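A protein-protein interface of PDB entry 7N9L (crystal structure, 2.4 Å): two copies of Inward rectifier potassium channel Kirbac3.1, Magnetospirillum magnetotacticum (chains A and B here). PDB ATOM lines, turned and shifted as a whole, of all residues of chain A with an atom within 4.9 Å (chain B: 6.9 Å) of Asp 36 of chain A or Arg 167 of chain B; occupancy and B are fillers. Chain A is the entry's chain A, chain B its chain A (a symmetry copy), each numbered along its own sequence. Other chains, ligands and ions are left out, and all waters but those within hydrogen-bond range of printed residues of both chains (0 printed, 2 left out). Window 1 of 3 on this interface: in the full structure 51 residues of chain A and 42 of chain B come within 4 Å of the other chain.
NH2 of Arg 25 of chain A lies within hydrogen-bond range of O of Arg 167 of chain B, 3.2 Å away.
The side-chain carboxylate of Asp 36 of chain A lies within salt-bridge range of the guanidinium group of Arg 167 of chain B, at 2.6 Å.
NE2 of His 39 of chain A sits at hydrogen-bond distance from OE1 of Glu 169 of chain B (2.6 Å).
The guanidinium group (NH2) of Arg 25 of chain A is in hydrogen-bond range of the backbone carbonyl oxygen (O) of Asn 165 of chain B (2.9 Å).
The guanidinium group of Arg 25 of chain A lies within hydrogen-bond range of the backbone carbonyl oxygen of Ser 209 of chain B (2.8 Å).
A ring nitrogen (ND1) of His 39 of chain A lies within hydrogen-bond range of the side-chain carboxylate of Asp 40 of chain A.
N of Arg 167 of chain B is in hydrogen-bond range of OD1 of Asn 165 of chain B (2.8 Å).
The backbone NH (N) of Asn 165 of chain B is in hydrogen-bond range of the backbone carbonyl oxygen (O) of Leu 210 of chain B, at 2.8 Å.
The backbone carbonyl oxygen (O) of Glu 169 of chain B sits at hydrogen-bond distance from the side-chain amide nitrogen (ND2) of Asn 165 of chain B, at 2.8 Å.
O of Ser 209 of chain B lies close to ND2 of Asn 165 of chain B (3.4 Å).
ND1 of His 247 of chain B lies within hydrogen-bond range of N of Ala 249 of chain B (3.2 Å).
Leu 210 of chain B touches Arg 25 of chain A (CD2 to NE, 3.4 Å).
Tyr 38 of chain A touches Phe 250 of chain B (CD2 to CE1, 3.7 Å).
CD2 of His 39 of chain A touches CD of Arg 167 of chain B, at 3.4 Å.
His 39 of chain A touches Ala 249 of chain B.
His 39 of chain A touches Phe 250 of chain B (CB to CZ, 3.7 Å).
Of the printed residues of chain B, Arg 25 of chain A touches Asn 165 (2.9 Å), Arg 167 (3.2 Å), Ser 209 (2.8 Å) and Leu 210 (3.4 Å).
Asp 36 of chain A touches just one residue of chain B: Arg 167.
Printed residues of chain A within 4 Å of Arg 167 of chain B: Arg 25 (3.2 Å), Asp 36 (2.6 Å) and His 39 (3.4 Å).
Of the printed residues of chain A, Ala 249 of chain B touches His 39 (3.5 Å).
Printed residues of chain A within 4 Å of Phe 250 of chain B: Tyr 38 (3.7 Å) and His 39 (3.7 Å).
The nearest residue of chain B that does not touch Asp 36 of chain A is Thr 139 of chain B (4.6 Å).
Printed residues of chain A that touch a printed residue of chain B: Arg 25, Asp 36, Tyr 38 and His 39.
Printed residues of chain B that touch a printed residue of chain A: Asn 165, Arg 167, Glu 169, Ser 209, Leu 210, Ala 249 and Phe 250.
Along chain B the printed residues that touch a printed residue of chain A span positions 165 to 250.
Among the printed residues, 10 pairs touch across the chains.
Among the printed residues, Asp or Glu carboxylates within 4 Å of a Lys or Arg side-chain nitrogen of the other chain: Asp 36 of chain A with Arg 167 of chain B.
No position is printed for both chains.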
ATOM      1  N   ARG A  25     -18.829  21.006 -18.890  1.00  0.00           N
ATOM      2  CA  ARG A  25     -17.855  22.068 -18.640  1.00  0.00           C
ATOM      3  C   ARG A  25     -16.755  22.032 -19.705  1.00  0.00           C
ATOM      4  O   ARG A  25     -15.597  21.681 -19.450  1.00  0.00           O
ATOM      5  CB  ARG A  25     -17.267  21.928 -17.241  1.00  0.00           C
ATOM      6  CG  ARG A  25     -18.160  22.398 -16.104  1.00  0.00           C
ATOM      7  CD  ARG A  25     -17.478  22.169 -14.756  1.00  0.00           C
ATOM      8  NE  ARG A  25     -17.913  23.115 -13.734  1.00  0.00           N
ATOM      9  CZ  ARG A  25     -17.338  24.289 -13.501  1.00  0.00           C
ATOM     10  NH1 ARG A  25     -16.301  24.705 -14.212  1.00  0.00           N
ATOM     11  NH2 ARG A  25     -17.817  25.066 -12.535  1.00  0.00           N
ATOM     12  N   LEU A  34       0.177  19.826 -11.727  1.00  0.00           N
ATOM     13  CA  LEU A  34       0.370  20.381 -10.392  1.00  0.00           C
ATOM     14  C   LEU A  34      -0.204  21.791 -10.267  1.00  0.00           C
ATOM     15  O   LEU A  34       0.240  22.565  -9.411  1.00  0.00           O
ATOM     16  CB  LEU A  34       1.854  20.387 -10.017  1.00  0.00           C
ATOM     17  CG  LEU A  34       2.570  19.051  -9.803  1.00  0.00           C
ATOM     18  CD1 LEU A  34       3.750  19.260  -8.856  1.00  0.00           C
ATOM     19  CD2 LEU A  34       1.655  17.963  -9.272  1.00  0.00           C
ATOM     20  N   ASP A  35      -1.183  22.144 -11.104  1.00  0.00           N
ATOM     21  CA  ASP A  35      -1.811  23.457 -11.018  1.00  0.00           C
ATOM     22  C   ASP A  35      -2.798  23.563  -9.861  1.00  0.00           C
ATOM     23  O   ASP A  35      -3.162  24.678  -9.472  1.00  0.00           O
ATOM     24  CB  ASP A  35      -2.523  23.778 -12.335  1.00  0.00           C
ATOM     25  CG  ASP A  35      -3.325  25.065 -12.270  1.00  0.00           C
ATOM     26  OD1 ASP A  35      -2.724  26.132 -12.021  1.00  0.00           O
ATOM     27  OD2 ASP A  35      -4.557  25.010 -12.470  1.00  0.00           O
ATOM     28  N   ASP A  36      -3.227  22.437  -9.299  1.00  0.00           N
ATOM     29  CA  ASP A  36      -4.193  22.424  -8.205  1.00  0.00           C
ATOM     30  C   ASP A  36      -3.884  21.221  -7.315  1.00  0.00           C
ATOM     31  O   ASP A  36      -4.770  20.452  -6.938  1.00  0.00           O
ATOM     32  CB  ASP A  36      -5.617  22.379  -8.759  1.00  0.00           C
ATOM     33  CG  ASP A  36      -6.640  23.023  -7.838  1.00  0.00           C
ATOM     34  OD1 ASP A  36      -6.258  23.755  -6.901  1.00  0.00           O
ATOM     35  OD2 ASP A  36      -7.843  22.787  -8.064  1.00  0.00           O
ATOM     36  N   HIS A  37      -2.604  21.046  -6.973  1.00  0.00           N
ATOM     37  CA  HIS A  37      -2.147  19.765  -6.442  1.00  0.00           C
ATOM     38  C   HIS A  37      -2.803  19.443  -5.107  1.00  0.00           C
ATOM     39  O   HIS A  37      -3.083  18.274  -4.813  1.00  0.00           O
ATOM     40  CB  HIS A  37      -0.622  19.759  -6.304  1.00  0.00           C
ATOM     41  CG  HIS A  37      -0.086  20.867  -5.453  1.00  0.00           C
ATOM     42  ND1 HIS A  37       0.287  22.089  -5.970  1.00  0.00           N
ATOM     43  CD2 HIS A  37       0.138  20.939  -4.119  1.00  0.00           C
ATOM     44  CE1 HIS A  37       0.714  22.867  -4.991  1.00  0.00           C
ATOM     45  NE2 HIS A  37       0.634  22.193  -3.858  1.00  0.00           N
ATOM     46  N   TYR A  38      -3.053  20.458  -4.280  1.00  0.00           N
ATOM     47  CA  TYR A  38      -3.653  20.189  -2.979  1.00  0.00           C
ATOM     48  C   TYR A  38      -5.092  19.714  -3.137  1.00  0.00           C
ATOM     49  O   TYR A  38      -5.505  18.729  -2.511  1.00  0.00           O
ATOM     50  CB  TYR A  38      -3.591  21.426  -2.084  1.00  0.00           C
ATOM     51  CG  TYR A  38      -4.229  21.180  -0.735  1.00  0.00           C
ATOM     52  CD1 TYR A  38      -3.698  20.242   0.139  1.00  0.00           C
ATOM     53  CD2 TYR A  38      -5.369  21.865  -0.344  1.00  0.00           C
ATOM     54  CE1 TYR A  38      -4.281  19.998   1.369  1.00  0.00           C
ATOM     55  CE2 TYR A  38      -5.959  21.629   0.888  1.00  0.00           C
ATOM     56  CZ  TYR A  38      -5.409  20.691   1.739  1.00  0.00           C
ATOM     57  OH  TYR A  38      -5.982  20.439   2.967  1.00  0.00           O
ATOM     58  N   HIS A  39      -5.871  20.405  -3.973  1.00  0.00           N
ATOM     59  CA  HIS A  39      -7.222  19.948  -4.275  1.00  0.00           C
ATOM     60  C   HIS A  39      -7.209  18.539  -4.853  1.00  0.00           C
ATOM     61  O   HIS A  39      -8.028  17.694  -4.474  1.00  0.00           O
ATOM     62  CB  HIS A  39      -7.892  20.920  -5.251  1.00  0.00           C
ATOM     63  CG  HIS A  39      -9.081  20.346  -5.958  1.00  0.00           C
ATOM     64  ND1 HIS A  39      -8.970  19.572  -7.093  1.00  0.00           N
ATOM     65  CD2 HIS A  39     -10.406  20.437  -5.694  1.00  0.00           C
ATOM     66  CE1 HIS A  39     -10.175  19.208  -7.495  1.00  0.00           C
ATOM     67  NE2 HIS A  39     -11.064  19.725  -6.667  1.00  0.00           N
ATOM     68  N   ASP A  40      -6.283  18.267  -5.773  1.00  0.00           N
ATOM     69  CA  ASP A  40      -6.268  16.968  -6.435  1.00  0.00           C
ATOM     70  C   ASP A  40      -5.938  15.849  -5.458  1.00  0.00           C
ATOM     71  O   ASP A  40      -6.471  14.741  -5.574  1.00  0.00           O
ATOM     72  CB  ASP A  40      -5.267  16.984  -7.588  1.00  0.00           C
ATOM     73  CG  ASP A  40      -5.595  18.036  -8.625  1.00  0.00           C
ATOM     74  OD1 ASP A  40      -6.775  18.441  -8.707  1.00  0.00           O
ATOM     75  OD2 ASP A  40      -4.675  18.456  -9.358  1.00  0.00           O
ATOM     76  N   PRO B 138      -7.007  25.921   2.022  1.00  0.00           N
ATOM     77  CA  PRO B 138      -7.359  25.810   0.600  1.00  0.00           C
ATOM     78  C   PRO B 138      -7.738  27.140  -0.026  1.00  0.00           C
ATOM     79  O   PRO B 138      -8.117  28.105   0.642  1.00  0.00           O
ATOM     80  CB  PRO B 138      -8.559  24.854   0.611  1.00  0.00           C
ATOM     81  CG  PRO B 138      -9.202  25.099   1.947  1.00  0.00           C
ATOM     82  CD  PRO B 138      -8.054  25.358   2.897  1.00  0.00           C
ATOM     83  N   THR B 139      -7.648  27.162  -1.354  1.00  0.00           N
ATOM     84  CA  THR B 139      -8.057  28.291  -2.173  1.00  0.00           C
ATOM     85  C   THR B 139      -9.474  28.066  -2.685  1.00  0.00           C
ATOM     86  O   THR B 139      -9.915  26.928  -2.869  1.00  0.00           O
ATOM     87  CB  THR B 139      -7.110  28.479  -3.356  1.00  0.00           C
ATOM     88  OG1 THR B 139      -7.279  27.398  -4.282  1.00  0.00           O
ATOM     89  CG2 THR B 139      -5.674  28.506  -2.882  1.00  0.00           C
ATOM     90  N   ALA B 140     -10.181  29.169  -2.929  1.00  0.00           N
ATOM     91  CA  ALA B 140     -11.575  29.072  -3.344  1.00  0.00           C
ATOM     92  C   ALA B 140     -11.716  28.548  -4.769  1.00  0.00           C
ATOM     93  O   ALA B 140     -12.724  27.910  -5.094  1.00  0.00           O
ATOM     94  CB  ALA B 140     -12.251  30.437  -3.216  1.00  0.00           C
ATOM     95  N   GLY B 141     -10.732  28.804  -5.626  1.00  0.00           N
ATOM     96  CA  GLY B 141     -10.841  28.415  -7.021  1.00  0.00           C
ATOM     97  C   GLY B 141     -11.876  29.216  -7.781  1.00  0.00           C
ATOM     98  O   GLY B 141     -12.567  28.668  -8.649  1.00  0.00           O
ATOM     99  N   VAL B 142     -11.995  30.505  -7.481  1.00  0.00           N
ATOM    100  CA  VAL B 142     -13.030  31.361  -8.044  1.00  0.00           C
ATOM    101  C   VAL B 142     -12.372  32.409  -8.927  1.00  0.00           C
ATOM    102  O   VAL B 142     -11.385  33.039  -8.530  1.00  0.00           O
ATOM    103  CB  VAL B 142     -13.872  32.019  -6.938  1.00  0.00           C
ATOM    104  CG1 VAL B 142     -14.743  33.112  -7.513  1.00  0.00           C
ATOM    105  CG2 VAL B 142     -14.715  30.966  -6.237  1.00  0.00           C
ATOM    106  N   ALA B 164     -16.837  32.905 -11.428  1.00  0.00           N
ATOM    107  CA  ALA B 164     -16.888  31.578 -12.021  1.00  0.00           C
ATOM    108  C   ALA B 164     -16.166  30.575 -11.134  1.00  0.00           C
ATOM    109  O   ALA B 164     -15.102  30.869 -10.584  1.00  0.00           O
ATOM    110  CB  ALA B 164     -16.266  31.574 -13.424  1.00  0.00           C
ATOM    111  N   ASN B 165     -16.753  29.388 -11.003  1.00  0.00           N
ATOM    112  CA  ASN B 165     -16.132  28.286 -10.280  1.00  0.00           C
ATOM    113  C   ASN B 165     -15.199  27.542 -11.229  1.00  0.00           C
ATOM    114  O   ASN B 165     -15.641  27.005 -12.250  1.00  0.00           O
ATOM    115  CB  ASN B 165     -17.189  27.338  -9.716  1.00  0.00           C
ATOM    116  CG  ASN B 165     -16.591  26.254  -8.834  1.00  0.00           C
ATOM    117  OD1 ASN B 165     -15.375  26.059  -8.811  1.00  0.00           O
ATOM    118  ND2 ASN B 165     -17.444  25.542  -8.107  1.00  0.00           N
ATOM    119  N   LEU B 166     -13.910  27.512 -10.891  1.00  0.00           N
ATOM    120  CA  LEU B 166     -12.910  26.868 -11.734  1.00  0.00           C
ATOM    121  C   LEU B 166     -12.800  25.371 -11.483  1.00  0.00           C
ATOM    122  O   LEU B 166     -11.991  24.708 -12.142  1.00  0.00           O
ATOM    123  CB  LEU B 166     -11.545  27.526 -11.514  1.00  0.00           C
ATOM    124  CG  LEU B 166     -11.459  28.996 -11.924  1.00  0.00           C
ATOM    125  CD1 LEU B 166     -10.112  29.573 -11.536  1.00  0.00           C
ATOM    126  CD2 LEU B 166     -11.700  29.161 -13.420  1.00  0.00           C
ATOM    127  N   ARG B 167     -13.590  24.827 -10.565  1.00  0.00           N
ATOM    128  CA  ARG B 167     -13.530  23.423 -10.202  1.00  0.00           C
ATOM    129  C   ARG B 167     -14.902  22.790 -10.380  1.00  0.00           C
ATOM    130  O   ARG B 167     -15.921  23.480 -10.468  1.00  0.00           O
ATOM    131  CB  ARG B 167     -13.063  23.244  -8.752  1.00  0.00           C
ATOM    132  CG  ARG B 167     -11.724  23.888  -8.448  1.00  0.00           C
ATOM    133  CD  ARG B 167     -11.204  23.408  -7.108  1.00  0.00           C
ATOM    134  NE  ARG B 167      -9.868  23.903  -6.800  1.00  0.00           N
ATOM    135  CZ  ARG B 167      -9.597  24.831  -5.890  1.00  0.00           C
ATOM    136  NH1 ARG B 167     -10.558  25.432  -5.202  1.00  0.00           N
ATOM    137  NH2 ARG B 167      -8.328  25.158  -5.656  1.00  0.00           N
ATOM    138  N   ILE B 168     -14.914  21.456 -10.424  1.00  0.00           N
ATOM    139  CA  ILE B 168     -16.171  20.742 -10.598  1.00  0.00           C
ATOM    140  C   ILE B 168     -16.945  20.615  -9.294  1.00  0.00           C
ATOM    141  O   ILE B 168     -18.163  20.403  -9.325  1.00  0.00           O
ATOM    142  CB  ILE B 168     -15.937  19.344 -11.196  1.00  0.00           C
ATOM    143  CG1 ILE B 168     -15.049  18.498 -10.281  1.00  0.00           C
ATOM    144  CG2 ILE B 168     -15.295  19.453 -12.573  1.00  0.00           C
ATOM    145  CD1 ILE B 168     -14.893  17.060 -10.744  1.00  0.00           C
ATOM    146  N   GLU B 169     -16.280  20.730  -8.147  1.00  0.00           N
ATOM    147  CA  GLU B 169     -16.964  20.611  -6.868  1.00  0.00           C
ATOM    148  C   GLU B 169     -17.684  21.912  -6.546  1.00  0.00           C
ATOM    149  O   GLU B 169     -17.195  23.004  -6.849  1.00  0.00           O
ATOM    150  CB  GLU B 169     -15.984  20.262  -5.749  1.00  0.00           C
ATOM    151  CG  GLU B 169     -15.353  18.882  -5.869  1.00  0.00           C
ATOM    152  CD  GLU B 169     -14.131  18.873  -6.768  1.00  0.00           C
ATOM    153  OE1 GLU B 169     -13.610  19.963  -7.079  1.00  0.00           O
ATOM    154  OE2 GLU B 169     -13.687  17.776  -7.164  1.00  0.00           O
ATOM    155  N   GLN B 170     -18.847  21.788  -5.922  1.00  0.00           N
ATOM    156  CA  GLN B 170     -19.720  22.925  -5.683  1.00  0.00           C
ATOM    157  C   GLN B 170     -19.382  23.599  -4.360  1.00  0.00           C
ATOM    158  O   GLN B 170     -18.764  23.011  -3.469  1.00  0.00           O
ATOM    159  CB  GLN B 170     -21.182  22.477  -5.700  1.00  0.00           C
ATOM    160  CG  GLN B 170     -21.581  21.767  -6.990  1.00  0.00           C
ATOM    161  CD  GLN B 170     -22.987  21.201  -6.940  1.00  0.00           C
ATOM    162  OE1 GLN B 170     -23.305  20.368  -6.090  1.00  0.00           O
ATOM    163  NE2 GLN B 170     -23.841  21.655  -7.854  1.00  0.00           N
ATOM    164  N   ILE B 171     -19.786  24.862  -4.251  1.00  0.00           N
ATOM    165  CA  ILE B 171     -19.535  25.686  -3.075  1.00  0.00           C
ATOM    166  C   ILE B 171     -20.879  26.028  -2.449  1.00  0.00           C
ATOM    167  O   ILE B 171     -21.767  26.561  -3.125  1.00  0.00           O
ATOM    168  CB  ILE B 171     -18.744  26.958  -3.434  1.00  0.00           C
ATOM    169  CG1 ILE B 171     -17.406  26.583  -4.081  1.00  0.00           C
ATOM    170  CG2 ILE B 171     -18.515  27.809  -2.192  1.00  0.00           C
ATOM    171  CD1 ILE B 171     -16.631  27.766  -4.639  1.00  0.00           C
ATOM    172  N   SER B 209     -22.223  26.678  -8.363  1.00  0.00           N
ATOM    173  CA  SER B 209     -21.642  25.579  -9.123  1.00  0.00           C
ATOM    174  C   SER B 209     -20.846  26.029 -10.335  1.00  0.00           C
ATOM    175  O   SER B 209     -19.794  25.451 -10.619  1.00  0.00           O
ATOM    176  CB  SER B 209     -22.750  24.624  -9.584  1.00  0.00           C
ATOM    177  OG  SER B 209     -22.212  23.542 -10.320  1.00  0.00           O
ATOM    178  N   LEU B 210     -21.311  27.049 -11.055  1.00  0.00           N
ATOM    179  CA  LEU B 210     -20.711  27.392 -12.337  1.00  0.00           C
ATOM    180  C   LEU B 210     -20.399  28.879 -12.437  1.00  0.00           C
ATOM    181  O   LEU B 210     -19.235  29.280 -12.331  1.00  0.00           O
ATOM    182  CB  LEU B 210     -21.648  26.967 -13.472  1.00  0.00           C
ATOM    183  CG  LEU B 210     -22.134  25.517 -13.395  1.00  0.00           C
ATOM    184  CD1 LEU B 210     -23.253  25.288 -14.392  1.00  0.00           C
ATOM    185  CD2 LEU B 210     -20.993  24.538 -13.634  1.00  0.00           C
ATOM    186  N   HIS B 247     -16.646  24.954   0.558  1.00  0.00           N
ATOM    187  CA  HIS B 247     -16.255  24.183  -0.613  1.00  0.00           C
ATOM    188  C   HIS B 247     -16.399  22.693  -0.333  1.00  0.00           C
ATOM    189  O   HIS B 247     -15.902  22.192   0.681  1.00  0.00           O
ATOM    190  CB  HIS B 247     -14.812  24.510  -1.005  1.00  0.00           C
ATOM    191  CG  HIS B 247     -14.533  24.346  -2.466  1.00  0.00           C
ATOM    192  ND1 HIS B 247     -14.623  23.132  -3.111  1.00  0.00           N
ATOM    193  CD2 HIS B 247     -14.163  25.246  -3.408  1.00  0.00           C
ATOM    194  CE1 HIS B 247     -14.327  23.292  -4.388  1.00  0.00           C
ATOM    195  NE2 HIS B 247     -14.045  24.566  -4.595  1.00  0.00           N
ATOM    196  N   ALA B 249     -15.118  20.190  -2.098  1.00  0.00           N
ATOM    197  CA  ALA B 249     -13.867  19.467  -2.288  1.00  0.00           C
ATOM    198  C   ALA B 249     -13.074  19.371  -0.990  1.00  0.00           C
ATOM    199  O   ALA B 249     -12.335  18.403  -0.786  1.00  0.00           O
ATOM    200  CB  ALA B 249     -13.031  20.144  -3.377  1.00  0.00           C
ATOM    201  N   PHE B 250     -13.223  20.353  -0.100  1.00  0.00           N
ATOM    202  CA  PHE B 250     -12.442  20.417   1.123  1.00  0.00           C
ATOM    203  C   PHE B 250     -13.276  20.266   2.386  1.00  0.00           C
ATOM    204  O   PHE B 250     -12.699  20.162   3.475  1.00  0.00           O
ATOM    205  CB  PHE B 250     -11.676  21.751   1.204  1.00  0.00           C
ATOM    206  CG  PHE B 250     -10.877  22.073  -0.032  1.00  0.00           C
ATOM    207  CD1 PHE B 250      -9.689  21.418  -0.295  1.00  0.00           C
ATOM    208  CD2 PHE B 250     -11.310  23.043  -0.924  1.00  0.00           C
ATOM    209  CE1 PHE B 250      -8.952  21.714  -1.426  1.00  0.00           C
ATOM    210  CE2 PHE B 250     -10.577  23.342  -2.056  1.00  0.00           C
ATOM    211  CZ  PHE B 250      -9.396  22.677  -2.308  1.00  0.00           C
ATOM    212  N   VAL B 254     -13.973  28.650   2.351  1.00  0.00           N
ATOM    213  CA  VAL B 254     -13.012  29.299   1.474  1.00  0.00           C
ATOM    214  C   VAL B 254     -13.478  30.731   1.242  1.00  0.00           C
ATOM    215  O   VAL B 254     -14.619  31.090   1.524  1.00  0.00           O
ATOM    216  CB  VAL B 254     -12.850  28.559   0.134  1.00  0.00           C
ATOM    217  CG1 VAL B 254     -12.284  27.167   0.364  1.00  0.00           C
ATOM    218  CG2 VAL B 254     -14.189  28.489  -0.589  1.00  0.00           C
